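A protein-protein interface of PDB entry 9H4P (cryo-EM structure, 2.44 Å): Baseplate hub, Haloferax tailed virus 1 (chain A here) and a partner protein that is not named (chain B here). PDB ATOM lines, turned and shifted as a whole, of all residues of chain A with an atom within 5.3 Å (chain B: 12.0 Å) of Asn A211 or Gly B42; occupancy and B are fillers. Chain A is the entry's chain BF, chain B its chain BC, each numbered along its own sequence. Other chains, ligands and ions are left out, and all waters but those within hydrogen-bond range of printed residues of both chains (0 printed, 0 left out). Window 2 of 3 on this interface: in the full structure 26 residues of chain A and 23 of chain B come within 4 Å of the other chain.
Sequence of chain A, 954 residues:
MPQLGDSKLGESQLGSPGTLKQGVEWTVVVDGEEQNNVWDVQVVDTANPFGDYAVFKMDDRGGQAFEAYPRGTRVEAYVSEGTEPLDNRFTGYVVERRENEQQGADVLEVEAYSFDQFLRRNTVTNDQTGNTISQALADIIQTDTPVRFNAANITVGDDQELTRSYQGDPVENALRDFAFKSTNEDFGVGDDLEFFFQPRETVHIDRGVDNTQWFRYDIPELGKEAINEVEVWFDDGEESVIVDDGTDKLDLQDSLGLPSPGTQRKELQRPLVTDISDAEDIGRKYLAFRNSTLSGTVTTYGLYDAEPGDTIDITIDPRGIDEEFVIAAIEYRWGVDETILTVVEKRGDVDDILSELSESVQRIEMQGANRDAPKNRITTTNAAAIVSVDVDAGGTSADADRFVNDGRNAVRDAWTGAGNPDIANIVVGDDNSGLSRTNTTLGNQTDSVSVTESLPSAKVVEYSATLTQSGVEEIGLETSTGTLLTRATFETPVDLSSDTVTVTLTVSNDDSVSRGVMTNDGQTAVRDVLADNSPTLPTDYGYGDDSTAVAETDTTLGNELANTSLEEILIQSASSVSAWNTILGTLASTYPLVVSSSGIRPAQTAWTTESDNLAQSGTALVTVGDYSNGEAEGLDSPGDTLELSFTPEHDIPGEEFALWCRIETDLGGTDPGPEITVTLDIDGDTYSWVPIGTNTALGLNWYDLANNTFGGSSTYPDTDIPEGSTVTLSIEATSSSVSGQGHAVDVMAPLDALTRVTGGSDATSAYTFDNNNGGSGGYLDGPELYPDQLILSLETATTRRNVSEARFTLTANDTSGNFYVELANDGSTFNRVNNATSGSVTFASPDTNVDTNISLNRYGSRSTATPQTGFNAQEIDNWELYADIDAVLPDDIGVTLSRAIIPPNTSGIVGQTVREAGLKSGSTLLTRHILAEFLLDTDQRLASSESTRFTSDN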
ATOM      1  N   VAL A 209      -0.994  -8.165 -16.807  1.00  0.00           N
ATOM      2  CA  VAL A 209      -0.261  -6.933 -17.120  1.00  0.00           C
ATOM      3  C   VAL A 209      -0.018  -6.860 -18.623  1.00  0.00           C
ATOM      4  O   VAL A 209       1.046  -7.195 -19.126  1.00  0.00           O
ATOM      5  CB  VAL A 209       1.038  -6.796 -16.311  1.00  0.00           C
ATOM      6  CG1 VAL A 209       1.644  -5.408 -16.511  1.00  0.00           C
ATOM      7  CG2 VAL A 209       0.790  -6.965 -14.815  1.00  0.00           C
ATOM      8  N   ASP A 210      -1.043  -6.453 -19.353  1.00  0.00           N
ATOM      9  CA  ASP A 210      -0.977  -6.150 -20.779  1.00  0.00           C
ATOM     10  C   ASP A 210       0.005  -5.008 -21.098  1.00  0.00           C
ATOM     11  O   ASP A 210       0.354  -4.211 -20.229  1.00  0.00           O
ATOM     12  CB  ASP A 210      -2.407  -5.844 -21.227  1.00  0.00           C
ATOM     13  CG  ASP A 210      -2.441  -5.072 -22.531  1.00  0.00           C
ATOM     14  OD1 ASP A 210      -2.125  -5.678 -23.575  1.00  0.00           O
ATOM     15  OD2 ASP A 210      -2.633  -3.839 -22.466  1.00  0.00           O
ATOM     16  N   ASN A 211       0.425  -4.877 -22.358  1.00  0.00           N
ATOM     17  CA  ASN A 211       1.410  -3.885 -22.780  1.00  0.00           C
ATOM     18  C   ASN A 211       1.015  -2.428 -22.485  1.00  0.00           C
ATOM     19  O   ASN A 211       1.868  -1.559 -22.386  1.00  0.00           O
ATOM     20  CB  ASN A 211       1.687  -4.081 -24.271  1.00  0.00           C
ATOM     21  CG  ASN A 211       2.909  -3.302 -24.695  1.00  0.00           C
ATOM     22  OD1 ASN A 211       3.938  -3.339 -24.046  1.00  0.00           O
ATOM     23  ND2 ASN A 211       2.836  -2.566 -25.774  1.00  0.00           N
ATOM     24  N   THR A 212      -0.267  -2.129 -22.318  1.00  0.00           N
ATOM     25  CA  THR A 212      -0.732  -0.792 -21.929  1.00  0.00           C
ATOM     26  C   THR A 212      -0.749  -0.573 -20.413  1.00  0.00           C
ATOM     27  O   THR A 212      -1.136   0.503 -19.968  1.00  0.00           O
ATOM     28  CB  THR A 212      -2.117  -0.522 -22.515  1.00  0.00           C
ATOM     29  OG1 THR A 212      -3.080  -1.351 -21.914  1.00  0.00           O
ATOM     30  CG2 THR A 212      -2.180  -0.723 -24.021  1.00  0.00           C
ATOM     31  N   GLN A 213      -0.382  -1.567 -19.599  1.00  0.00           N
ATOM     32  CA  GLN A 213      -0.623  -1.600 -18.151  1.00  0.00           C
ATOM     33  C   GLN A 213       0.634  -1.703 -17.284  1.00  0.00           C
ATOM     34  O   GLN A 213       0.526  -1.587 -16.066  1.00  0.00           O
ATOM     35  CB  GLN A 213      -1.580  -2.751 -17.808  1.00  0.00           C
ATOM     36  CG  GLN A 213      -2.857  -2.727 -18.653  1.00  0.00           C
ATOM     37  CD  GLN A 213      -4.030  -3.406 -17.975  1.00  0.00           C
ATOM     38  OE1 GLN A 213      -4.551  -2.924 -16.986  1.00  0.00           O
ATOM     39  NE2 GLN A 213      -4.546  -4.492 -18.484  1.00  0.00           N
ATOM     40  N   TRP A 214       1.808  -1.923 -17.861  1.00  0.00           N
ATOM     41  CA  TRP A 214       3.080  -1.748 -17.169  1.00  0.00           C
ATOM     42  C   TRP A 214       3.537  -0.293 -17.274  1.00  0.00           C
ATOM     43  O   TRP A 214       3.246   0.372 -18.259  1.00  0.00           O
ATOM     44  CB  TRP A 214       4.121  -2.710 -17.744  1.00  0.00           C
ATOM     45  CG  TRP A 214       4.560  -2.405 -19.134  1.00  0.00           C
ATOM     46  CD1 TRP A 214       4.018  -2.900 -20.263  1.00  0.00           C
ATOM     47  CD2 TRP A 214       5.584  -1.471 -19.571  1.00  0.00           C
ATOM     48  NE1 TRP A 214       4.609  -2.309 -21.357  1.00  0.00           N
ATOM     49  CE2 TRP A 214       5.553  -1.385 -20.987  1.00  0.00           C
ATOM     50  CE3 TRP A 214       6.533  -0.679 -18.901  1.00  0.00           C
ATOM     51  CZ2 TRP A 214       6.377  -0.513 -21.701  1.00  0.00           C
ATOM     52  CZ3 TRP A 214       7.372   0.199 -19.609  1.00  0.00           C
ATOM     53  CH2 TRP A 214       7.281   0.296 -21.000  1.00  0.00           C
ATOM     54  N   THR A 315       2.781  -8.979 -20.605  1.00  0.00           N
ATOM     55  CA  THR A 315       3.262  -8.602 -21.929  1.00  0.00           C
ATOM     56  C   THR A 315       3.994  -7.277 -21.834  1.00  0.00           C
ATOM     57  O   THR A 315       3.410  -6.293 -21.395  1.00  0.00           O
ATOM     58  CB  THR A 315       2.093  -8.479 -22.910  1.00  0.00           C
ATOM     59  OG1 THR A 315       1.266  -9.614 -22.884  1.00  0.00           O
ATOM     60  CG2 THR A 315       2.572  -8.285 -24.340  1.00  0.00           C
ATOM     61  N   ILE A 316       5.253  -7.210 -22.252  1.00  0.00           N
ATOM     62  CA  ILE A 316       6.031  -5.970 -22.258  1.00  0.00           C
ATOM     63  C   ILE A 316       6.849  -5.874 -23.536  1.00  0.00           C
ATOM     64  O   ILE A 316       7.868  -6.539 -23.699  1.00  0.00           O
ATOM     65  CB  ILE A 316       6.936  -5.829 -21.017  1.00  0.00           C
ATOM     66  CG1 ILE A 316       6.170  -6.032 -19.706  1.00  0.00           C
ATOM     67  CG2 ILE A 316       7.639  -4.464 -21.018  1.00  0.00           C
ATOM     68  CD1 ILE A 316       7.012  -5.819 -18.451  1.00  0.00           C
ATOM     69  N   ASP A 317       6.471  -4.938 -24.391  1.00  0.00           N
ATOM     70  CA  ASP A 317       7.312  -4.426 -25.468  1.00  0.00           C
ATOM     71  C   ASP A 317       7.825  -3.032 -25.057  1.00  0.00           C
ATOM     72  O   ASP A 317       7.038  -2.224 -24.571  1.00  0.00           O
ATOM     73  CB  ASP A 317       6.499  -4.345 -26.761  1.00  0.00           C
ATOM     74  CG  ASP A 317       5.675  -5.602 -27.055  1.00  0.00           C
ATOM     75  OD1 ASP A 317       6.184  -6.721 -26.839  1.00  0.00           O
ATOM     76  OD2 ASP A 317       4.541  -5.466 -27.560  1.00  0.00           O
ATOM     77  N   VAL B  37       0.246  10.941 -13.388  1.00  0.00           N
ATOM     78  CA  VAL B  37       0.413  10.699 -14.815  1.00  0.00           C
ATOM     79  C   VAL B  37       1.651   9.814 -14.975  1.00  0.00           C
ATOM     80  O   VAL B  37       2.736  10.200 -14.537  1.00  0.00           O
ATOM     81  CB  VAL B  37       0.544  12.020 -15.609  1.00  0.00           C
ATOM     82  CG1 VAL B  37       0.763  11.796 -17.102  1.00  0.00           C
ATOM     83  CG2 VAL B  37      -0.635  12.959 -15.376  1.00  0.00           C
ATOM     84  N   ARG B  38       1.485   8.630 -15.584  1.00  0.00           N
ATOM     85  CA  ARG B  38       2.581   7.679 -15.753  1.00  0.00           C
ATOM     86  C   ARG B  38       3.577   8.219 -16.783  1.00  0.00           C
ATOM     87  O   ARG B  38       3.172   8.649 -17.865  1.00  0.00           O
ATOM     88  CB  ARG B  38       2.038   6.300 -16.153  1.00  0.00           C
ATOM     89  CG  ARG B  38       1.522   5.453 -14.996  1.00  0.00           C
ATOM     90  CD  ARG B  38       0.521   6.145 -14.081  1.00  0.00           C
ATOM     91  NE  ARG B  38      -0.293   5.252 -13.270  1.00  0.00           N
ATOM     92  CZ  ARG B  38      -0.074   4.921 -11.997  1.00  0.00           C
ATOM     93  NH1 ARG B  38      -0.921   4.106 -11.392  1.00  0.00           N
ATOM     94  NH2 ARG B  38       0.965   5.398 -11.333  1.00  0.00           N
ATOM     95  N   LYS B  39       4.878   8.176 -16.446  1.00  0.00           N
ATOM     96  CA  LYS B  39       5.935   8.748 -17.275  1.00  0.00           C
ATOM     97  C   LYS B  39       6.243   7.876 -18.499  1.00  0.00           C
ATOM     98  O   LYS B  39       6.832   8.365 -19.466  1.00  0.00           O
ATOM     99  CB  LYS B  39       7.195   9.020 -16.445  1.00  0.00           C
ATOM    100  CG  LYS B  39       7.070  10.175 -15.457  1.00  0.00           C
ATOM    101  CD  LYS B  39       8.313  10.444 -14.647  1.00  0.00           C
ATOM    102  CE  LYS B  39       9.448  11.002 -15.475  1.00  0.00           C
ATOM    103  NZ  LYS B  39      10.599  11.375 -14.625  1.00  0.00           N
ATOM    104  N   SER B  40       5.834   6.595 -18.451  1.00  0.00           N
ATOM    105  CA  SER B  40       6.167   5.580 -19.446  1.00  0.00           C
ATOM    106  C   SER B  40       5.030   4.551 -19.550  1.00  0.00           C
ATOM    107  O   SER B  40       3.943   4.780 -19.018  1.00  0.00           O
ATOM    108  CB  SER B  40       7.505   4.950 -19.105  1.00  0.00           C
ATOM    109  OG  SER B  40       8.013   4.183 -20.186  1.00  0.00           O
ATOM    110  N   GLY B  41       5.286   3.418 -20.230  1.00  0.00           N
ATOM    111  CA  GLY B  41       4.267   2.432 -20.585  1.00  0.00           C
ATOM    112  C   GLY B  41       4.056   2.365 -22.102  1.00  0.00           C
ATOM    113  O   GLY B  41       4.431   3.300 -22.808  1.00  0.00           O
ATOM    114  N   GLY B  42       3.425   1.285 -22.595  1.00  0.00           N
ATOM    115  CA  GLY B  42       3.387   0.968 -24.019  1.00  0.00           C
ATOM    116  C   GLY B  42       2.295   1.666 -24.841  1.00  0.00           C
ATOM    117  O   GLY B  42       2.199   1.409 -26.042  1.00  0.00           O
ATOM    118  N   SER B  43       1.489   2.547 -24.216  1.00  0.00           N
ATOM    119  CA  SER B  43       0.434   3.313 -24.883  1.00  0.00           C
ATOM    120  C   SER B  43       1.014   4.556 -25.565  1.00  0.00           C
ATOM    121  O   SER B  43       2.092   4.997 -25.183  1.00  0.00           O
ATOM    122  CB  SER B  43      -0.625   3.730 -23.890  1.00  0.00           C
ATOM    123  OG  SER B  43      -1.196   2.608 -23.236  1.00  0.00           O
ATOM    124  N   LEU B  44       0.287   5.143 -26.537  1.00  0.00           N
ATOM    125  CA  LEU B  44       0.663   6.429 -27.124  1.00  0.00           C
ATOM    126  C   LEU B  44       0.488   7.568 -26.113  1.00  0.00           C
ATOM    127  O   LEU B  44       1.308   8.486 -26.072  1.00  0.00           O
ATOM    128  CB  LEU B  44      -0.133   6.715 -28.406  1.00  0.00           C
ATOM    129  CG  LEU B  44       0.499   6.244 -29.721  1.00  0.00           C
ATOM    130  CD1 LEU B  44      -0.462   6.447 -30.883  1.00  0.00           C
ATOM    131  CD2 LEU B  44       1.829   6.935 -30.009  1.00  0.00           C
ATOM    132  N   ASN B  45      -0.592   7.507 -25.315  1.00  0.00           N
ATOM    133  CA  ASN B  45      -0.919   8.508 -24.308  1.00  0.00           C
ATOM    134  C   ASN B  45      -0.945   7.823 -22.935  1.00  0.00           C
ATOM    135  O   ASN B  45      -1.337   6.655 -22.852  1.00  0.00           O
ATOM    136  CB  ASN B  45      -2.239   9.222 -24.638  1.00  0.00           C
ATOM    137  CG  ASN B  45      -2.378   9.642 -26.089  1.00  0.00           C
ATOM    138  OD1 ASN B  45      -1.542  10.374 -26.618  1.00  0.00           O
ATOM    139  ND2 ASN B  45      -3.445   9.198 -26.736  1.00  0.00           N
ATOM    140  N   PRO B  46      -0.539   8.498 -21.821  1.00  0.00           N
ATOM    141  CA  PRO B  46      -0.370   7.816 -20.531  1.00  0.00           C
ATOM    142  C   PRO B  46      -1.686   7.441 -19.846  1.00  0.00           C
ATOM    143  O   PRO B  46      -2.697   8.130 -20.002  1.00  0.00           O
ATOM    144  CB  PRO B  46       0.385   8.851 -19.673  1.00  0.00           C
ATOM    145  CG  PRO B  46      -0.034  10.198 -20.244  1.00  0.00           C
ATOM    146  CD  PRO B  46      -0.230   9.941 -21.726  1.00  0.00           C
ATOM    147  N   ARG B  47      -1.649   6.339 -19.085  1.00  0.00           N
ATOM    148  CA  ARG B  47      -2.649   6.095 -18.058  1.00  0.00           C
ATOM    149  C   ARG B  47      -2.422   7.063 -16.898  1.00  0.00           C
ATOM    150  O   ARG B  47      -1.290   7.479 -16.640  1.00  0.00           O
ATOM    151  CB  ARG B  47      -2.594   4.646 -17.571  1.00  0.00           C
ATOM    152  CG  ARG B  47      -3.420   3.696 -18.424  1.00  0.00           C
ATOM    153  CD  ARG B  47      -3.491   2.306 -17.822  1.00  0.00           C
ATOM    154  NE  ARG B  47      -4.720   1.619 -18.211  1.00  0.00           N
ATOM    155  CZ  ARG B  47      -4.882   0.830 -19.275  1.00  0.00           C
ATOM    156  NH1 ARG B  47      -6.060   0.271 -19.500  1.00  0.00           N
ATOM    157  NH2 ARG B  47      -3.883   0.593 -20.105  1.00  0.00           N
ATOM    158  N   VAL B  48      -3.519   7.403 -16.201  1.00  0.00           N
ATOM    159  CA  VAL B  48      -3.513   8.377 -15.117  1.00  0.00           C
ATOM    160  C   VAL B  48      -4.368   7.860 -13.955  1.00  0.00           C
ATOM    161  O   VAL B  48      -5.175   6.942 -14.129  1.00  0.00           O
ATOM    162  CB  VAL B  48      -3.989   9.772 -15.591  1.00  0.00           C
ATOM    163  CG1 VAL B  48      -3.136  10.344 -16.718  1.00  0.00           C
ATOM    164  CG2 VAL B  48      -5.469   9.807 -15.970  1.00  0.00           C
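The backbone carbonyl oxygen of Asn A211 lies within hydrogen-bond range of the backbone NH of Gly B42, at 3.2 Å.
O of Thr A212 is in hydrogen-bond range of NH2 of Arg B47, at 2.8 Å.
Asn A211 touches one residue of chain B.
Of chain A, only Asn A211 and Trp A214 come within 4 Å of Gly B42.
No residue of chain B comes within 4 Å of Val A209.
Asp A210 touches none of the printed residues of chain B.
Gln A213 touches just one residue of chain B: Arg B47.
Of chain B, only Gly B41 (3.3 Å) and Gly B42 (3.6 Å) come within 4 Å of Trp A214.
No residue of chain B comes within 4 Å of Asp A317.
Of the printed residues of chain A, Arg B47 touches Thr A212 (2.8 Å) and Gln A213 (3.8 Å).
Of the printed residues of chain A, Gly B41 touches Trp A214.
Among the printed residues, merely in contact across the chains: Thr A212 with Ser B43 (3.3 Å), Gln A213 with Arg B47 (3.8 Å), Trp A214 with Gly B41 (3.3 Å) and Trp A214 with Gly B42 (3.6 Å).
The backbone carbonyl oxygen of Thr A315 lies close to the backbone NH of Asn A211, at 3.4 Å.
The side-chain amide oxygen of Asn A211 lies within hydrogen-bond range of the backbone NH of Asp A317.
The backbone NH (N) of Arg B38 sits at hydrogen-bond distance from the backbone carbonyl oxygen (O) of Arg B47, 3.2 Å away.
The side-chain amide oxygen of Asn A211 lies within hydrogen-bond range of the indole nitrogen of Trp A214 (3.0 Å).
OD2 of Asp A210 lies within hydrogen-bond range of OG1 of Thr A212 (2.6 Å).
Printed residues of chain B that touch a printed residue of chain A: Gly B41, Gly B42, Ser B43 and Arg B47.
Of the 9 printed residues of chain A, 4 touch a printed residue of chain B.
Hydrophobic or aromatic side chains of chain A within 4 Å of the printed part of chain B: Trp A214.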
